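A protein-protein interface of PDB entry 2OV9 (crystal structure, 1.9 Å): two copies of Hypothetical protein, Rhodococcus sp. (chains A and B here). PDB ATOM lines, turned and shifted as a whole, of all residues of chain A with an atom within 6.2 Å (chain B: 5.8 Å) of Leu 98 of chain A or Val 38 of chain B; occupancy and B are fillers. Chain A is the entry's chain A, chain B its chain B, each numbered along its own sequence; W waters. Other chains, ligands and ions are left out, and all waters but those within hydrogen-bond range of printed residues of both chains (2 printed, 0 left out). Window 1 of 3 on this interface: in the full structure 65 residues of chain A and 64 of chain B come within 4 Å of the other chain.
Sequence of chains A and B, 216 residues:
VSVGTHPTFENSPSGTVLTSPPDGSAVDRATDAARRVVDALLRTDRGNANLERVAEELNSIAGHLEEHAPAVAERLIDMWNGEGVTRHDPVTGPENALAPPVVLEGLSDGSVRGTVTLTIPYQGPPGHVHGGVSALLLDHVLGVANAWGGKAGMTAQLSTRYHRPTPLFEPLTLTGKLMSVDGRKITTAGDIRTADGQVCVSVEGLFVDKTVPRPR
The backbone carbonyl oxygen of Pro 121 of chain B sits at hydrogen-bond distance from the side-chain amide nitrogen of Asn 96 of chain A (2.8 Å).
O of Leu 98 of chain A is in hydrogen-bond range of OH of Tyr 122 of chain A, at 2.7 Å. The side-chain amide nitrogen of Asn 96 of chain A sits close to the backbone carbonyl oxygen of Asp 89 of chain A, at 3.5 Å. The backbone carbonyl oxygen of Leu 98 of chain B is in hydrogen-bond range of the side-chain hydroxyl of Tyr 122 of chain B (2.7 Å). The side-chain amide oxygen of Asn 96 of chain A lies within hydrogen-bond range of the backbone NH of Leu 98 of chain A, at 2.9 Å. NH1 of Arg 35 of chain A is in hydrogen-bond range of O of Asn 96 of chain A (2.9 Å).
CA of Thr 31 of chain A touches CD1 of Leu 41 of chain B, at 3.9 Å. CD1 of Leu 41 of chain B touches CB of Ala 34 of chain A, at 3.7 Å. Val 38 of chain A touches Ala 97 of chain B (CG2 to CB, 3.9 Å). Pro 121 of chain B touches Pro 90 of chain A (O to CB, 3.2 Å). O of Glu 95 of chain A touches CD2 of Leu 42 of chain B, at 3.5 Å. Asn 96 of chain A touches Leu 42 of chain B (CB to CD2, 3.8 Å). Val 38 of chain B touches Ala 97 of chain A (CG2 to CB, 3.7 Å). CD1 of Leu 98 of chain A touches CG1 of Val 38 of chain B, at 3.6 Å. Leu 98 of chain A touches Pro 121 of chain B (CD2 to CB, 3.3 Å). Tyr 122 of chain A touches Leu 98 of chain B.
Of the printed residues of chain B, Asn 96 of chain A touches Leu 42 and Pro 121. Of the printed residues of chain B, Ala 97 of chain A touches Val 38. Of chain A, only Ala 97 (3.7 Å) and Leu 98 (3.6 Å) come within 4 Å of Val 38 of chain B. Of the printed residues of chain A, Pro 121 of chain B touches Pro 90, Asn 96 and Leu 98. Printed residues of chain A within 4 Å of Tyr 122 of chain B: Leu 98 (3.5 Å). The nearest residue of chain B that does not touch Leu 98 of chain A is Leu 98 of chain B (4.1 Å).
Hydrophobic or aromatic side chains of chain B that line the printed part of chain A: Val 38, Leu 41, Leu 42, Ala 97, Leu 98, Pro 121 and Tyr 122. Of the 14 printed residues of chain A, 9 touch a printed residue of chain B. Hydrophobic or aromatic side chains of chain A within 4 Å of the printed part of chain B: Ala 34, Val 38, Pro 90, Ala 97, Leu 98 and Tyr 122. Along chain A the printed residues that touch a printed residue of chain B span positions 31 to 122. Among the printed residues, 13 pairs touch across the chains.
Val 38 of chain A touches Ala 97 of chain B, and with the chains exchanged Ala 97 of chain A touches Val 38 of chain B. Val 38 of chain A touches Leu 98 of chain B, and with the chains exchanged Leu 98 of chain A touches Val 38 of chain B. Leu 98 of chain A touches Tyr 122 of chain B, and with the chains exchanged Tyr 122 of chain A touches Leu 98 of chain B. Positions printed for both chains: 34, 35, 38, 97, 98 and 122. Of the 13 pairs that touch across the chains among the printed residues, 6 have their exchanged pair printed and touching as well.
Water W2 lies within hydrogen-bond range of the backbone carbonyl oxygen (O) of Val 38 of chain B, the backbone carbonyl oxygen (O) of Glu 95 of chain A and the backbone NH (N) of Ala 97 of chain A. Water W1 lies within hydrogen-bond range of O of Val 38 of chain A and N of Ala 97 of chain B.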
ATOM      1  N   THR A  31      27.274   9.961 -11.750  1.00  0.00           N
ATOM      2  CA  THR A  31      27.140   9.266 -13.031  1.00  0.00           C
ATOM      3  C   THR A  31      26.609   7.850 -12.803  1.00  0.00           C
ATOM      4  O   THR A  31      25.723   7.382 -13.532  1.00  0.00           O
ATOM      5  CB  THR A  31      28.456   9.215 -13.813  1.00  0.00           C
ATOM      6  OG1 THR A  31      28.957  10.546 -13.983  1.00  0.00           O
ATOM      7  CG2 THR A  31      28.206   8.611 -15.185  1.00  0.00           C
ATOM      8  N   ALA A  34      23.067   8.163 -12.350  1.00  0.00           N
ATOM      9  CA  ALA A  34      22.411   8.323 -13.666  1.00  0.00           C
ATOM     10  C   ALA A  34      22.266   6.996 -14.438  1.00  0.00           C
ATOM     11  O   ALA A  34      21.245   6.745 -15.102  1.00  0.00           O
ATOM     12  CB  ALA A  34      23.150   9.354 -14.508  1.00  0.00           C
ATOM     13  N   ARG A  35      23.291   6.155 -14.360  1.00  0.00           N
ATOM     14  CA  ARG A  35      23.245   4.845 -14.992  1.00  0.00           C
ATOM     15  C   ARG A  35      22.094   4.026 -14.393  1.00  0.00           C
ATOM     16  O   ARG A  35      21.381   3.322 -15.118  1.00  0.00           O
ATOM     17  CB  ARG A  35      24.605   4.126 -14.888  1.00  0.00           C
ATOM     18  CG  ARG A  35      25.617   4.670 -15.925  1.00  0.00           C
ATOM     19  CD  ARG A  35      26.998   3.967 -16.076  1.00  0.00           C
ATOM     20  NE  ARG A  35      27.861   4.429 -15.018  1.00  0.00           N
ATOM     21  CZ  ARG A  35      29.008   5.088 -15.132  1.00  0.00           C
ATOM     22  NH1 ARG A  35      29.589   5.373 -16.299  1.00  0.00           N
ATOM     23  NH2 ARG A  35      29.590   5.445 -14.007  1.00  0.00           N
ATOM     24  N   VAL A  38      18.771   5.355 -15.847  1.00  0.00           N
ATOM     25  CA  VAL A  38      18.655   4.860 -17.232  1.00  0.00           C
ATOM     26  C   VAL A  38      18.087   3.428 -17.269  1.00  0.00           C
ATOM     27  O   VAL A  38      17.152   3.118 -18.032  1.00  0.00           O
ATOM     28  CB  VAL A  38      20.024   4.934 -17.969  1.00  0.00           C
ATOM     29  CG1 VAL A  38      19.980   4.204 -19.330  1.00  0.00           C
ATOM     30  CG2 VAL A  38      20.448   6.402 -18.142  1.00  0.00           C
ATOM     31  N   ASP A  89      34.808   8.303 -23.333  1.00  0.00           N
ATOM     32  CA  ASP A  89      34.115   7.503 -24.331  1.00  0.00           C
ATOM     33  C   ASP A  89      32.937   6.720 -23.744  1.00  0.00           C
ATOM     34  O   ASP A  89      32.848   6.524 -22.529  1.00  0.00           O
ATOM     35  CB  ASP A  89      35.075   6.490 -24.945  1.00  0.00           C
ATOM     36  CG  ASP A  89      35.552   5.511 -23.919  1.00  0.00           C
ATOM     37  OD1 ASP A  89      36.431   5.889 -23.110  1.00  0.00           O
ATOM     38  OD2 ASP A  89      35.023   4.379 -23.903  1.00  0.00           O
ATOM     39  N   PRO A  90      31.998   6.325 -24.616  1.00  0.00           N
ATOM     40  CA  PRO A  90      30.805   5.610 -24.196  1.00  0.00           C
ATOM     41  C   PRO A  90      31.024   4.119 -23.942  1.00  0.00           C
ATOM     42  O   PRO A  90      30.041   3.364 -23.844  1.00  0.00           O
ATOM     43  CB  PRO A  90      29.838   5.851 -25.363  1.00  0.00           C
ATOM     44  CG  PRO A  90      30.713   5.968 -26.559  1.00  0.00           C
ATOM     45  CD  PRO A  90      31.968   6.647 -26.060  1.00  0.00           C
ATOM     46  N   VAL A  91      32.281   3.695 -23.811  1.00  0.00           N
ATOM     47  CA  VAL A  91      32.588   2.304 -23.404  1.00  0.00           C
ATOM     48  C   VAL A  91      33.225   2.255 -22.000  1.00  0.00           C
ATOM     49  O   VAL A  91      32.845   1.412 -21.166  1.00  0.00           O
ATOM     50  CB  VAL A  91      33.484   1.579 -24.458  1.00  0.00           C
ATOM     51  CG1 VAL A  91      33.781   0.106 -24.052  1.00  0.00           C
ATOM     52  CG2 VAL A  91      32.820   1.617 -25.850  1.00  0.00           C
ATOM     53  N   GLU A  95      32.596   9.153 -16.289  1.00  0.00           N
ATOM     54  CA  GLU A  95      31.570  10.180 -16.225  1.00  0.00           C
ATOM     55  C   GLU A  95      30.561  10.117 -17.380  1.00  0.00           C
ATOM     56  O   GLU A  95      29.700  10.982 -17.482  1.00  0.00           O
ATOM     57  CB  GLU A  95      32.201  11.560 -16.145  1.00  0.00           C
ATOM     58  CG  GLU A  95      32.926  11.810 -14.839  1.00  0.00           C
ATOM     59  CD  GLU A  95      34.269  12.447 -15.066  1.00  0.00           C
ATOM     60  OE1 GLU A  95      34.602  12.732 -16.234  1.00  0.00           O
ATOM     61  OE2 GLU A  95      35.006  12.659 -14.077  1.00  0.00           O
ATOM     62  N   ASN A  96      30.650   9.066 -18.197  1.00  0.00           N
ATOM     63  CA  ASN A  96      29.755   8.860 -19.332  1.00  0.00           C
ATOM     64  C   ASN A  96      28.739   7.786 -18.968  1.00  0.00           C
ATOM     65  O   ASN A  96      29.065   6.606 -18.896  1.00  0.00           O
ATOM     66  CB  ASN A  96      30.557   8.502 -20.597  1.00  0.00           C
ATOM     67  CG  ASN A  96      29.706   8.515 -21.857  1.00  0.00           C
ATOM     68  OD1 ASN A  96      28.521   8.211 -21.806  1.00  0.00           O
ATOM     69  ND2 ASN A  96      30.323   8.829 -23.005  1.00  0.00           N
ATOM     70  N   ALA A  97      27.503   8.204 -18.707  1.00  0.00           N
ATOM     71  CA  ALA A  97      26.478   7.265 -18.261  1.00  0.00           C
ATOM     72  C   ALA A  97      26.063   6.262 -19.339  1.00  0.00           C
ATOM     73  O   ALA A  97      25.353   5.288 -19.052  1.00  0.00           O
ATOM     74  CB  ALA A  97      25.265   8.008 -17.704  1.00  0.00           C
ATOM     75  N   LEU A  98      26.513   6.490 -20.575  1.00  0.00           N
ATOM     76  CA  LEU A  98      26.279   5.518 -21.640  1.00  0.00           C
ATOM     77  C   LEU A  98      27.210   4.333 -21.520  1.00  0.00           C
ATOM     78  O   LEU A  98      26.882   3.263 -22.022  1.00  0.00           O
ATOM     79  CB  LEU A  98      26.432   6.148 -23.022  1.00  0.00           C
ATOM     80  CG  LEU A  98      25.240   6.780 -23.727  1.00  0.00           C
ATOM     81  CD1 LEU A  98      24.327   7.540 -22.834  1.00  0.00           C
ATOM     82  CD2 LEU A  98      25.729   7.642 -24.886  1.00  0.00           C
ATOM     83  N   ALA A  99      28.361   4.532 -20.867  1.00  0.00           N
ATOM     84  CA  ALA A  99      29.336   3.457 -20.666  1.00  0.00           C
ATOM     85  C   ALA A  99      28.869   2.518 -19.563  1.00  0.00           C
ATOM     86  O   ALA A  99      28.320   2.968 -18.577  1.00  0.00           O
ATOM     87  CB  ALA A  99      30.713   4.033 -20.342  1.00  0.00           C
ATOM     88  N   PRO A 100      29.052   1.201 -19.731  1.00  0.00           N
ATOM     89  CA  PRO A 100      28.678   0.316 -18.644  1.00  0.00           C
ATOM     90  C   PRO A 100      29.129   0.743 -17.223  1.00  0.00           C
ATOM     91  O   PRO A 100      28.301   0.689 -16.313  1.00  0.00           O
ATOM     92  CB  PRO A 100      29.239  -1.040 -19.079  1.00  0.00           C
ATOM     93  CG  PRO A 100      29.193  -0.968 -20.560  1.00  0.00           C
ATOM     94  CD  PRO A 100      29.494   0.452 -20.923  1.00  0.00           C
ATOM     95  N   TYR A 122      21.389  -2.271 -22.957  1.00  0.00           N
ATOM     96  CA  TYR A 122      22.226  -2.783 -24.062  1.00  0.00           C
ATOM     97  C   TYR A 122      21.572  -3.913 -24.853  1.00  0.00           C
ATOM     98  O   TYR A 122      22.197  -4.481 -25.758  1.00  0.00           O
ATOM     99  CB  TYR A 122      23.627  -3.199 -23.549  1.00  0.00           C
ATOM    100  CG  TYR A 122      24.311  -2.088 -22.792  1.00  0.00           C
ATOM    101  CD1 TYR A 122      25.045  -1.112 -23.462  1.00  0.00           C
ATOM    102  CD2 TYR A 122      24.141  -1.963 -21.403  1.00  0.00           C
ATOM    103  CE1 TYR A 122      25.642  -0.045 -22.749  1.00  0.00           C
ATOM    104  CE2 TYR A 122      24.738  -0.915 -20.686  1.00  0.00           C
ATOM    105  CZ  TYR A 122      25.477   0.041 -21.367  1.00  0.00           C
ATOM    106  OH  TYR A 122      26.056   1.073 -20.656  1.00  0.00           O
ATOM    107  N   ALA B  33      14.614  13.771 -20.233  1.00  0.00           N
ATOM    108  CA  ALA B  33      15.264  14.499 -19.148  1.00  0.00           C
ATOM    109  C   ALA B  33      16.529  13.764 -18.695  1.00  0.00           C
ATOM    110  O   ALA B  33      17.563  14.398 -18.454  1.00  0.00           O
ATOM    111  CB  ALA B  33      14.307  14.669 -17.994  1.00  0.00           C
ATOM    112  N   ALA B  34      16.453  12.434 -18.581  1.00  0.00           N
ATOM    113  CA  ALA B  34      17.641  11.613 -18.361  1.00  0.00           C
ATOM    114  C   ALA B  34      18.724  11.807 -19.411  1.00  0.00           C
ATOM    115  O   ALA B  34      19.908  11.930 -19.063  1.00  0.00           O
ATOM    116  CB  ALA B  34      17.279  10.119 -18.245  1.00  0.00           C
ATOM    117  N   ARG B  35      18.345  11.846 -20.688  1.00  0.00           N
ATOM    118  CA  ARG B  35      19.328  12.071 -21.753  1.00  0.00           C
ATOM    119  C   ARG B  35      20.024  13.413 -21.529  1.00  0.00           C
ATOM    120  O   ARG B  35      21.219  13.562 -21.788  1.00  0.00           O
ATOM    121  CB  ARG B  35      18.655  12.067 -23.137  1.00  0.00           C
ATOM    122  CG  ARG B  35      18.108  10.708 -23.571  1.00  0.00           C
ATOM    123  CD  ARG B  35      17.631  10.725 -25.063  1.00  0.00           C
ATOM    124  NE  ARG B  35      17.111   9.418 -25.431  1.00  0.00           N
ATOM    125  CZ  ARG B  35      15.823   9.108 -25.424  1.00  0.00           C
ATOM    126  NH1 ARG B  35      14.917  10.038 -25.114  1.00  0.00           N
ATOM    127  NH2 ARG B  35      15.435   7.889 -25.733  1.00  0.00           N
ATOM    128  N   ARG B  36      19.256  14.383 -21.054  1.00  0.00           N
ATOM    129  CA  ARG B  36      19.770  15.736 -20.839  1.00  0.00           C
ATOM    130  C   ARG B  36      20.774  15.745 -19.667  1.00  0.00           C
ATOM    131  O   ARG B  36      21.791  16.447 -19.710  1.00  0.00           O
ATOM    132  CB  ARG B  36      18.590  16.680 -20.580  1.00  0.00           C
ATOM    133  CG  ARG B  36      18.963  18.106 -20.428  1.00  0.00           C
ATOM    134  CD  ARG B  36      17.796  18.924 -19.906  1.00  0.00           C
ATOM    135  NE  ARG B  36      18.239  20.268 -19.559  1.00  0.00           N
ATOM    136  CZ  ARG B  36      17.453  21.195 -19.026  1.00  0.00           C
ATOM    137  NH1 ARG B  36      16.162  20.925 -18.772  1.00  0.00           N
ATOM    138  NH2 ARG B  36      17.954  22.399 -18.750  1.00  0.00           N
ATOM    139  N   VAL B  37      20.465  14.980 -18.631  1.00  0.00           N
ATOM    140  CA  VAL B  37      21.358  14.773 -17.487  1.00  0.00           C
ATOM    141  C   VAL B  37      22.683  14.093 -17.919  1.00  0.00           C
ATOM    142  O   VAL B  37      23.773  14.548 -17.523  1.00  0.00           O
ATOM    143  CB  VAL B  37      20.677  13.914 -16.376  1.00  0.00           C
ATOM    144  CG1 VAL B  37      21.703  13.437 -15.339  1.00  0.00           C
ATOM    145  CG2 VAL B  37      19.521  14.664 -15.707  1.00  0.00           C
ATOM    146  N   VAL B  38      22.573  13.000 -18.682  1.00  0.00           N
ATOM    147  CA  VAL B  38      23.734  12.291 -19.252  1.00  0.00           C
ATOM    148  C   VAL B  38      24.644  13.242 -20.026  1.00  0.00           C
ATOM    149  O   VAL B  38      25.847  13.265 -19.794  1.00  0.00           O
ATOM    150  CB  VAL B  38      23.313  11.104 -20.144  1.00  0.00           C
ATOM    151  CG1 VAL B  38      24.527  10.529 -20.923  1.00  0.00           C
ATOM    152  CG2 VAL B  38      22.606  10.012 -19.296  1.00  0.00           C
ATOM    153  N   ASP B  39      24.079  14.036 -20.930  1.00  0.00           N
ATOM    154  CA  ASP B  39      24.867  15.056 -21.633  1.00  0.00           C
ATOM    155  C   ASP B  39      25.567  16.034 -20.661  1.00  0.00           C
ATOM    156  O   ASP B  39      26.778  16.282 -20.782  1.00  0.00           O
ATOM    157  CB  ASP B  39      23.963  15.842 -22.591  1.00  0.00           C
ATOM    158  CG  ASP B  39      24.747  16.640 -23.600  1.00  0.00           C
ATOM    159  OD1 ASP B  39      25.068  16.117 -24.670  1.00  0.00           O
ATOM    160  OD2 ASP B  39      25.075  17.809 -23.316  1.00  0.00           O
ATOM    161  N   ALA B  40      24.801  16.584 -19.710  1.00  0.00           N
ATOM    162  CA  ALA B  40      25.287  17.645 -18.814  1.00  0.00           C
ATOM    163  C   ALA B  40      26.430  17.193 -17.899  1.00  0.00           C
ATOM    164  O   ALA B  40      27.345  17.966 -17.623  1.00  0.00           O
ATOM    165  CB  ALA B  40      24.130  18.217 -17.974  1.00  0.00           C
ATOM    166  N   LEU B  41      26.355  15.942 -17.446  1.00  0.00           N
ATOM    167  CA  LEU B  41      27.387  15.332 -16.590  1.00  0.00           C
ATOM    168  C   LEU B  41      28.746  15.333 -17.255  1.00  0.00           C
ATOM    169  O   LEU B  41      29.763  15.484 -16.593  1.00  0.00           O
ATOM    170  CB  LEU B  41      26.997  13.885 -16.213  1.00  0.00           C
ATOM    171  CG  LEU B  41      26.022  13.643 -15.046  1.00  0.00           C
ATOM    172  CD1 LEU B  41      25.527  12.165 -14.999  1.00  0.00           C
ATOM    173  CD2 LEU B  41      26.668  14.001 -13.724  1.00  0.00           C
ATOM    174  N   LEU B  42      28.775  15.180 -18.579  1.00  0.00           N
ATOM    175  CA  LEU B  42      30.061  15.158 -19.298  1.00  0.00           C
ATOM    176  C   LEU B  42      30.664  16.550 -19.482  1.00  0.00           C
ATOM    177  O   LEU B  42      31.850  16.692 -19.779  1.00  0.00           O
ATOM    178  CB  LEU B  42      29.910  14.460 -20.654  1.00  0.00           C
ATOM    179  CG  LEU B  42      29.805  12.939 -20.568  1.00  0.00           C
ATOM    180  CD1 LEU B  42      29.121  12.373 -21.793  1.00  0.00           C
ATOM    181  CD2 LEU B  42      31.190  12.287 -20.377  1.00  0.00           C
ATOM    182  N   ALA B  97      17.508   5.707 -22.612  1.00  0.00           N
ATOM    183  CA  ALA B  97      18.266   6.949 -22.611  1.00  0.00           C
ATOM    184  C   ALA B  97      19.635   6.839 -23.284  1.00  0.00           C
ATOM    185  O   ALA B  97      20.253   7.867 -23.577  1.00  0.00           O
ATOM    186  CB  ALA B  97      18.384   7.553 -21.193  1.00  0.00           C
ATOM    187  N   LEU B  98      20.073   5.611 -23.573  1.00  0.00           N
ATOM    188  CA  LEU B  98      21.274   5.381 -24.403  1.00  0.00           C
ATOM    189  C   LEU B  98      21.054   5.731 -25.856  1.00  0.00           C
ATOM    190  O   LEU B  98      22.023   6.022 -26.563  1.00  0.00           O
ATOM    191  CB  LEU B  98      21.703   3.899 -24.377  1.00  0.00           C
ATOM    192  CG  LEU B  98      22.675   3.499 -23.257  1.00  0.00           C
ATOM    193  CD1 LEU B  98      22.106   3.803 -21.940  1.00  0.00           C
ATOM    194  CD2 LEU B  98      23.000   2.000 -23.353  1.00  0.00           C
ATOM    195  N   PRO B 121      28.065  12.457 -25.434  1.00  0.00           N
ATOM    196  CA  PRO B 121      28.207  11.077 -24.914  1.00  0.00           C
ATOM    197  C   PRO B 121      28.671  10.067 -25.946  1.00  0.00           C
ATOM    198  O   PRO B 121      29.225   9.014 -25.570  1.00  0.00           O
ATOM    199  CB  PRO B 121      26.776  10.740 -24.463  1.00  0.00           C
ATOM    200  CG  PRO B 121      26.219  12.037 -24.063  1.00  0.00           C
ATOM    201  CD  PRO B 121      26.704  12.960 -25.173  1.00  0.00           C
ATOM    202  N   TYR B 122      28.411  10.370 -27.222  1.00  0.00           N
ATOM    203  CA  TYR B 122      28.751   9.504 -28.383  1.00  0.00           C
ATOM    204  C   TYR B 122      30.171   9.732 -28.956  1.00  0.00           C
ATOM    205  O   TYR B 122      30.562   9.122 -29.981  1.00  0.00           O
ATOM    206  CB  TYR B 122      27.663   9.667 -29.479  1.00  0.00           C
ATOM    207  CG  TYR B 122      26.278   9.358 -28.933  1.00  0.00           C
ATOM    208  CD1 TYR B 122      25.858   8.043 -28.746  1.00  0.00           C
ATOM    209  CD2 TYR B 122      25.435  10.381 -28.501  1.00  0.00           C
ATOM    210  CE1 TYR B 122      24.584   7.747 -28.218  1.00  0.00           C
ATOM    211  CE2 TYR B 122      24.180  10.105 -27.940  1.00  0.00           C
ATOM    212  CZ  TYR B 122      23.771   8.795 -27.806  1.00  0.00           C
ATOM    213  OH  TYR B 122      22.538   8.531 -27.281  1.00  0.00           O
HETATM  214  O   HOH W   1      16.400   4.637 -20.232  1.00  0.00           O
HETATM  215  O   HOH W   2      27.049  11.135 -18.593  1.00  0.00           O
